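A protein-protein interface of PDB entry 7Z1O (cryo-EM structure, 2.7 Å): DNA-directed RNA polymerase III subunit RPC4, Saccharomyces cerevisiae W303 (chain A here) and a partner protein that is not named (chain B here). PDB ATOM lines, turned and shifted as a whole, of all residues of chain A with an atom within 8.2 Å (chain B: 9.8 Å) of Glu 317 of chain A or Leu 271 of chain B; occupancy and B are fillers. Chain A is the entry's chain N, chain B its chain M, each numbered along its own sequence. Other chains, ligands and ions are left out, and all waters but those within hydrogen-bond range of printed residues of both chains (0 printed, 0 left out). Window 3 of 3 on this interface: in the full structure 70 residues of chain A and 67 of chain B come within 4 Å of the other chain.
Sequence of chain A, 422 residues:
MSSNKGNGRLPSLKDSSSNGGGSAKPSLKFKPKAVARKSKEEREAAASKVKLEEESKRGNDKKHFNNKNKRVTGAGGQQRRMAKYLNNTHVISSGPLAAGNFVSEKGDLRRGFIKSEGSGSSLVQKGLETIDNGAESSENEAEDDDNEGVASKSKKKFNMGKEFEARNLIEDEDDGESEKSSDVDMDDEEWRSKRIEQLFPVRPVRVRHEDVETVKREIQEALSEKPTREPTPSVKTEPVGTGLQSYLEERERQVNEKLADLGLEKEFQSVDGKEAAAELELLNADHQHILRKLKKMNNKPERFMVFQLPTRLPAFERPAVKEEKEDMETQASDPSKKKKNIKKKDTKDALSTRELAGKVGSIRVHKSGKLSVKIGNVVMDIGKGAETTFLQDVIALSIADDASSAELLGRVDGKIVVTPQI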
ATOM      1  N   PRO A 314      -7.300  11.455   5.973  1.00  0.00           N
ATOM      2  CA  PRO A 314      -5.973  12.027   6.245  1.00  0.00           C
ATOM      3  C   PRO A 314      -5.063  11.032   6.946  1.00  0.00           C
ATOM      4  O   PRO A 314      -5.507  10.215   7.757  1.00  0.00           O
ATOM      5  CB  PRO A 314      -6.285  13.231   7.140  1.00  0.00           C
ATOM      6  CG  PRO A 314      -7.671  13.603   6.787  1.00  0.00           C
ATOM      7  CD  PRO A 314      -8.381  12.329   6.460  1.00  0.00           C
ATOM      8  N   ALA A 315      -3.777  11.103   6.611  1.00  0.00           N
ATOM      9  CA  ALA A 315      -2.819  10.108   7.073  1.00  0.00           C
ATOM     10  C   ALA A 315      -2.586  10.220   8.574  1.00  0.00           C
ATOM     11  O   ALA A 315      -2.477  11.318   9.127  1.00  0.00           O
ATOM     12  CB  ALA A 315      -1.495  10.264   6.324  1.00  0.00           C
ATOM     13  N   PHE A 316      -2.512   9.066   9.230  1.00  0.00           N
ATOM     14  CA  PHE A 316      -2.186   8.961  10.643  1.00  0.00           C
ATOM     15  C   PHE A 316      -0.937   8.104  10.785  1.00  0.00           C
ATOM     16  O   PHE A 316      -0.848   7.027  10.188  1.00  0.00           O
ATOM     17  CB  PHE A 316      -3.342   8.339  11.433  1.00  0.00           C
ATOM     18  CG  PHE A 316      -4.496   9.274  11.662  1.00  0.00           C
ATOM     19  CD1 PHE A 316      -4.462  10.203  12.688  1.00  0.00           C
ATOM     20  CD2 PHE A 316      -5.617   9.217  10.854  1.00  0.00           C
ATOM     21  CE1 PHE A 316      -5.527  11.059  12.900  1.00  0.00           C
ATOM     22  CE2 PHE A 316      -6.683  10.068  11.061  1.00  0.00           C
ATOM     23  CZ  PHE A 316      -6.638  10.991  12.085  1.00  0.00           C
ATOM     24  N   GLU A 317       0.032   8.585  11.562  1.00  0.00           N
ATOM     25  CA  GLU A 317       1.288   7.857  11.698  1.00  0.00           C
ATOM     26  C   GLU A 317       1.084   6.567  12.483  1.00  0.00           C
ATOM     27  O   GLU A 317       0.199   6.474  13.338  1.00  0.00           O
ATOM     28  CB  GLU A 317       2.355   8.732  12.362  1.00  0.00           C
ATOM     29  CG  GLU A 317       2.130   9.065  13.826  1.00  0.00           C
ATOM     30  CD  GLU A 317       1.232  10.271  14.027  1.00  0.00           C
ATOM     31  OE1 GLU A 317       0.538  10.679  13.072  1.00  0.00           O
ATOM     32  OE2 GLU A 317       1.243  10.830  15.141  1.00  0.00           O
ATOM     33  N   ARG A 318       1.903   5.568  12.167  1.00  0.00           N
ATOM     34  CA  ARG A 318       1.742   4.240  12.731  1.00  0.00           C
ATOM     35  C   ARG A 318       2.069   4.241  14.224  1.00  0.00           C
ATOM     36  O   ARG A 318       2.985   4.941  14.668  1.00  0.00           O
ATOM     37  CB  ARG A 318       2.645   3.251  11.999  1.00  0.00           C
ATOM     38  CG  ARG A 318       2.139   2.871  10.618  1.00  0.00           C
ATOM     39  CD  ARG A 318       3.290   2.515   9.692  1.00  0.00           C
ATOM     40  NE  ARG A 318       3.903   3.709   9.123  1.00  0.00           N
ATOM     41  CZ  ARG A 318       4.503   3.757   7.941  1.00  0.00           C
ATOM     42  NH1 ARG A 318       4.588   2.688   7.165  1.00  0.00           N
ATOM     43  NH2 ARG A 318       5.031   4.906   7.528  1.00  0.00           N
ATOM     44  N   PRO A 319       1.325   3.466  15.028  1.00  0.00           N
ATOM     45  CA  PRO A 319       1.565   3.354  16.471  1.00  0.00           C
ATOM     46  C   PRO A 319       2.911   2.713  16.795  1.00  0.00           C
ATOM     47  O   PRO A 319       3.191   2.471  17.968  1.00  0.00           O
ATOM     48  CB  PRO A 319       0.413   2.464  16.953  1.00  0.00           C
ATOM     49  CG  PRO A 319      -0.636   2.586  15.901  1.00  0.00           C
ATOM     50  CD  PRO A 319       0.114   2.734  14.617  1.00  0.00           C
ATOM     51  N   ALA A 350       0.744   7.565   6.064  1.00  0.00           N
ATOM     52  CA  ALA A 350       1.380   6.432   6.724  1.00  0.00           C
ATOM     53  C   ALA A 350       0.445   5.229   6.763  1.00  0.00           C
ATOM     54  O   ALA A 350       0.650   4.248   6.048  1.00  0.00           O
ATOM     55  CB  ALA A 350       1.816   6.813   8.128  1.00  0.00           C
ATOM     56  N   LEU A 351      -0.580   5.308   7.606  1.00  0.00           N
ATOM     57  CA  LEU A 351      -1.554   4.232   7.705  1.00  0.00           C
ATOM     58  C   LEU A 351      -2.451   4.204   6.473  1.00  0.00           C
ATOM     59  O   LEU A 351      -2.754   5.238   5.871  1.00  0.00           O
ATOM     60  CB  LEU A 351      -2.401   4.390   8.966  1.00  0.00           C
ATOM     61  CG  LEU A 351      -1.955   3.584  10.187  1.00  0.00           C
ATOM     62  CD1 LEU A 351      -2.897   3.812  11.360  1.00  0.00           C
ATOM     63  CD2 LEU A 351      -1.859   2.105   9.850  1.00  0.00           C
ATOM     64  N   ILE A 375     -11.564  15.614  11.319  1.00  0.00           N
ATOM     65  CA  ILE A 375     -10.791  14.383  11.204  1.00  0.00           C
ATOM     66  C   ILE A 375      -9.320  14.762  11.185  1.00  0.00           C
ATOM     67  O   ILE A 375      -8.886  15.542  10.329  1.00  0.00           O
ATOM     68  CB  ILE A 375     -11.168  13.588   9.942  1.00  0.00           C
ATOM     69  CG1 ILE A 375     -12.663  13.272   9.930  1.00  0.00           C
ATOM     70  CG2 ILE A 375     -10.360  12.306   9.867  1.00  0.00           C
ATOM     71  CD1 ILE A 375     -13.135  12.531  11.155  1.00  0.00           C
ATOM     72  N   GLY A 376      -8.556  14.219  12.127  1.00  0.00           N
ATOM     73  CA  GLY A 376      -7.159  14.578  12.241  1.00  0.00           C
ATOM     74  C   GLY A 376      -6.969  16.053  12.530  1.00  0.00           C
ATOM     75  O   GLY A 376      -7.237  16.516  13.643  1.00  0.00           O
ATOM     76  N   ASN A 377      -6.507  16.800  11.528  1.00  0.00           N
ATOM     77  CA  ASN A 377      -6.371  18.246  11.637  1.00  0.00           C
ATOM     78  C   ASN A 377      -7.232  19.004  10.634  1.00  0.00           C
ATOM     79  O   ASN A 377      -7.114  20.231  10.544  1.00  0.00           O
ATOM     80  CB  ASN A 377      -4.906  18.667  11.466  1.00  0.00           C
ATOM     81  CG  ASN A 377      -4.030  18.230  12.621  1.00  0.00           C
ATOM     82  OD1 ASN A 377      -4.453  18.243  13.778  1.00  0.00           O
ATOM     83  ND2 ASN A 377      -2.793  17.856  12.316  1.00  0.00           N
ATOM     84  N   THR B 267      -6.031   5.325  20.572  1.00  0.00           N
ATOM     85  CA  THR B 267      -6.237   6.750  20.342  1.00  0.00           C
ATOM     86  C   THR B 267      -5.151   7.243  19.400  1.00  0.00           C
ATOM     87  O   THR B 267      -3.961   7.144  19.717  1.00  0.00           O
ATOM     88  CB  THR B 267      -6.208   7.541  21.654  1.00  0.00           C
ATOM     89  OG1 THR B 267      -7.261   7.085  22.513  1.00  0.00           O
ATOM     90  CG2 THR B 267      -6.388   9.027  21.384  1.00  0.00           C
ATOM     91  N   LEU B 268      -5.556   7.768  18.249  1.00  0.00           N
ATOM     92  CA  LEU B 268      -4.634   8.205  17.215  1.00  0.00           C
ATOM     93  C   LEU B 268      -4.551   9.726  17.171  1.00  0.00           C
ATOM     94  O   LEU B 268      -5.554  10.427  17.327  1.00  0.00           O
ATOM     95  CB  LEU B 268      -5.056   7.668  15.845  1.00  0.00           C
ATOM     96  CG  LEU B 268      -4.494   6.315  15.399  1.00  0.00           C
ATOM     97  CD1 LEU B 268      -4.944   5.181  16.306  1.00  0.00           C
ATOM     98  CD2 LEU B 268      -4.893   6.033  13.959  1.00  0.00           C
ATOM     99  N   VAL B 269      -3.336  10.228  16.957  1.00  0.00           N
ATOM    100  CA  VAL B 269      -3.073  11.659  16.841  1.00  0.00           C
ATOM    101  C   VAL B 269      -2.686  11.962  15.399  1.00  0.00           C
ATOM    102  O   VAL B 269      -2.159  11.093  14.693  1.00  0.00           O
ATOM    103  CB  VAL B 269      -1.988  12.118  17.830  1.00  0.00           C
ATOM    104  CG1 VAL B 269      -2.474  11.937  19.259  1.00  0.00           C
ATOM    105  CG2 VAL B 269      -0.712  11.335  17.620  1.00  0.00           C
ATOM    106  N   ALA B 270      -2.944  13.193  14.968  1.00  0.00           N
ATOM    107  CA  ALA B 270      -2.913  13.525  13.551  1.00  0.00           C
ATOM    108  C   ALA B 270      -1.493  13.709  13.032  1.00  0.00           C
ATOM    109  O   ALA B 270      -0.555  13.944  13.799  1.00  0.00           O
ATOM    110  CB  ALA B 270      -3.717  14.797  13.298  1.00  0.00           C
ATOM    111  N   LEU B 271      -1.344  13.595  11.711  1.00  0.00           N
ATOM    112  CA  LEU B 271      -0.082  13.862  11.030  1.00  0.00           C
ATOM    113  C   LEU B 271      -0.198  15.000  10.024  1.00  0.00           C
ATOM    114  O   LEU B 271       0.586  15.951  10.085  1.00  0.00           O
ATOM    115  CB  LEU B 271       0.422  12.584  10.341  1.00  0.00           C
ATOM    116  CG  LEU B 271       1.765  12.653   9.607  1.00  0.00           C
ATOM    117  CD1 LEU B 271       2.605  11.433   9.921  1.00  0.00           C
ATOM    118  CD2 LEU B 271       1.560  12.765   8.102  1.00  0.00           C
ATOM    119  N   GLU B 272      -1.154  14.932   9.100  1.00  0.00           N
ATOM    120  CA  GLU B 272      -1.178  15.837   7.960  1.00  0.00           C
ATOM    121  C   GLU B 272      -1.700  17.218   8.337  1.00  0.00           C
ATOM    122  O   GLU B 272      -2.560  17.370   9.210  1.00  0.00           O
ATOM    123  CB  GLU B 272      -2.034  15.259   6.833  1.00  0.00           C
ATOM    124  CG  GLU B 272      -1.337  14.192   6.010  1.00  0.00           C
ATOM    125  CD  GLU B 272      -2.123  13.808   4.772  1.00  0.00           C
ATOM    126  OE1 GLU B 272      -3.269  14.280   4.625  1.00  0.00           O
ATOM    127  OE2 GLU B 272      -1.594  13.035   3.946  1.00  0.00           O
ATOM    128  N   LYS B 273      -1.165  18.228   7.660  1.00  0.00           N
ATOM    129  CA  LYS B 273      -1.632  19.599   7.774  1.00  0.00           C
ATOM    130  C   LYS B 273      -2.923  19.768   6.972  1.00  0.00           C
ATOM    131  O   LYS B 273      -3.270  18.935   6.128  1.00  0.00           O
ATOM    132  CB  LYS B 273      -0.540  20.560   7.287  1.00  0.00           C
ATOM    133  CG  LYS B 273      -0.735  22.035   7.628  1.00  0.00           C
ATOM    134  CD  LYS B 273       0.429  22.876   7.130  1.00  0.00           C
ATOM    135  CE  LYS B 273       0.279  24.329   7.550  1.00  0.00           C
ATOM    136  NZ  LYS B 273      -0.871  24.986   6.868  1.00  0.00           N
ATOM    137  N   GLN B 274      -3.649  20.852   7.260  1.00  0.00           N
ATOM    138  CA  GLN B 274      -4.903  21.123   6.563  1.00  0.00           C
ATOM    139  C   GLN B 274      -4.674  21.356   5.073  1.00  0.00           C
ATOM    140  O   GLN B 274      -5.454  20.892   4.234  1.00  0.00           O
ATOM    141  CB  GLN B 274      -5.602  22.328   7.195  1.00  0.00           C
ATOM    142  CG  GLN B 274      -7.117  22.220   7.218  1.00  0.00           C
ATOM    143  CD  GLN B 274      -7.764  22.859   6.007  1.00  0.00           C
ATOM    144  OE1 GLN B 274      -7.188  23.743   5.374  1.00  0.00           O
ATOM    145  NE2 GLN B 274      -8.971  22.412   5.676  1.00  0.00           N
ATOM    146  N   GLU B 275      -3.607  22.080   4.725  1.00  0.00           N
ATOM    147  CA  GLU B 275      -3.335  22.368   3.320  1.00  0.00           C
ATOM    148  C   GLU B 275      -2.863  21.124   2.577  1.00  0.00           C
ATOM    149  O   GLU B 275      -3.125  20.970   1.377  1.00  0.00           O
ATOM    150  CB  GLU B 275      -2.299  23.485   3.207  1.00  0.00           C
ATOM    151  CG  GLU B 275      -2.889  24.886   3.257  1.00  0.00           C
ATOM    152  CD  GLU B 275      -4.199  24.997   2.502  1.00  0.00           C
ATOM    153  OE1 GLU B 275      -4.183  24.874   1.259  1.00  0.00           O
ATOM    154  OE2 GLU B 275      -5.244  25.208   3.151  1.00  0.00           O
ATOM    155  N   ASP B 276      -2.163  20.223   3.274  1.00  0.00           N
ATOM    156  CA  ASP B 276      -1.644  19.020   2.629  1.00  0.00           C
ATOM    157  C   ASP B 276      -2.772  18.106   2.165  1.00  0.00           C
ATOM    158  O   ASP B 276      -2.623  17.379   1.176  1.00  0.00           O
ATOM    159  CB  ASP B 276      -0.709  18.277   3.583  1.00  0.00           C
ATOM    160  CG  ASP B 276       0.096  17.199   2.885  1.00  0.00           C
ATOM    161  OD1 ASP B 276       0.819  17.526   1.920  1.00  0.00           O
ATOM    162  OD2 ASP B 276       0.004  16.025   3.300  1.00  0.00           O
ATOM    163  N   TYR B 277      -3.904  18.120   2.871  1.00  0.00           N
ATOM    164  CA  TYR B 277      -5.054  17.339   2.429  1.00  0.00           C
ATOM    165  C   TYR B 277      -5.669  17.930   1.167  1.00  0.00           C
ATOM    166  O   TYR B 277      -6.123  17.193   0.285  1.00  0.00           O
ATOM    167  CB  TYR B 277      -6.096  17.251   3.540  1.00  0.00           C
ATOM    168  CG  TYR B 277      -7.142  16.196   3.284  1.00  0.00           C
ATOM    169  CD1 TYR B 277      -6.776  14.883   3.027  1.00  0.00           C
ATOM    170  CD2 TYR B 277      -8.490  16.515   3.275  1.00  0.00           C
ATOM    171  CE1 TYR B 277      -7.726  13.914   2.784  1.00  0.00           C
ATOM    172  CE2 TYR B 277      -9.446  15.555   3.030  1.00  0.00           C
ATOM    173  CZ  TYR B 277      -9.058  14.256   2.785  1.00  0.00           C
ATOM    174  OH  TYR B 277     -10.007  13.292   2.542  1.00  0.00           O
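ND2 of Asn 377 of chain A lies within hydrogen-bond range of O of Glu 272 of chain B (3.2 Å).
O of Val 269 of chain B sits close to OE1 of Glu 317 of chain A (3.2 Å).
O of Phe 316 of chain A lies within hydrogen-bond range of N of Leu 351 of chain A (3.1 Å).
The side-chain amide oxygen (OE1) of Gln 274 of chain B lies close to the side-chain carboxylate (OE2) of Glu 275 of chain B, at 3.3 Å.
Among the printed residues, pairs that only touch across the chains: Pro 314 of chain A with Glu 272 of chain B (3.9 Å), Ala 315 of chain A with Leu 271 of chain B (3.4 Å), Ala 315 of chain A with Glu 272 of chain B (3.7 Å), Phe 316 of chain A with Leu 268 of chain B (3.8 Å), Phe 316 of chain A with Val 269 of chain B (3.2 Å), Phe 316 of chain A with Ala 270 of chain B (3.7 Å), Glu 317 of chain A with Ala 270 of chain B (3.5 Å), Glu 317 of chain A with Leu 271 of chain B (3.3 Å), Leu 351 of chain A with Leu 268 of chain B (3.96 Å), Gly 376 of chain A with Ala 270 of chain B (3.6 Å), Asn 377 of chain A with Ala 270 of chain B (3.3 Å) and Asn 377 of chain A with Gln 274 of chain B (3.9 Å).
Glu 317 of chain A touches just these residues of chain B: Val 269 (3.2 Å), Ala 270 (3.5 Å) and Leu 271 (3.3 Å).
Printed residues of chain B within 4 Å of Leu 351 of chain A: Leu 268.
Printed residues of chain B within 4 Å of Asn 377 of chain A: Ala 270, Glu 272 and Gln 274.
Thr 267 of chain B touches none of the printed residues of chain A.
Of the printed residues of chain A, Leu 268 of chain B touches Phe 316 (3.8 Å) and Leu 351 (3.96 Å).
Leu 271 of chain B touches just these residues of chain A: Ala 315 (3.4 Å) and Glu 317 (3.3 Å).
Tyr 277 of chain B touches none of the printed residues of chain A.
The nearest printed residue of chain A that does not touch Leu 271 of chain B is Phe 316 of chain A (4.5 Å).
The nearest printed residue of chain B that does not touch Ala 315 of chain A is Ala 270 of chain B (4.7 Å).
Of the 11 printed residues of chain A, 7 touch a printed residue of chain B.
Printed residues of chain A that touch a printed residue of chain B: Pro 314, Ala 315, Phe 316, Glu 317, Leu 351, Gly 376 and Asn 377.
Hydrophobic or aromatic side chains of chain A that line the printed part of chain B: Ala 315, Phe 316 and Leu 351.
Printed residues of chain B that touch a printed residue of chain A: Leu 268, Val 269, Ala 270, Leu 271, Glu 272 and Gln 274.
Hydrophobic or aromatic side chains of chain B within 4 Å of the printed part of chain A: Leu 268, Val 269, Ala 270 and Leu 271.
Among the printed residues, no Asp or Glu carboxylate lies within 4 Å of a Lys or Arg side-chain nitrogen of the other chain.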
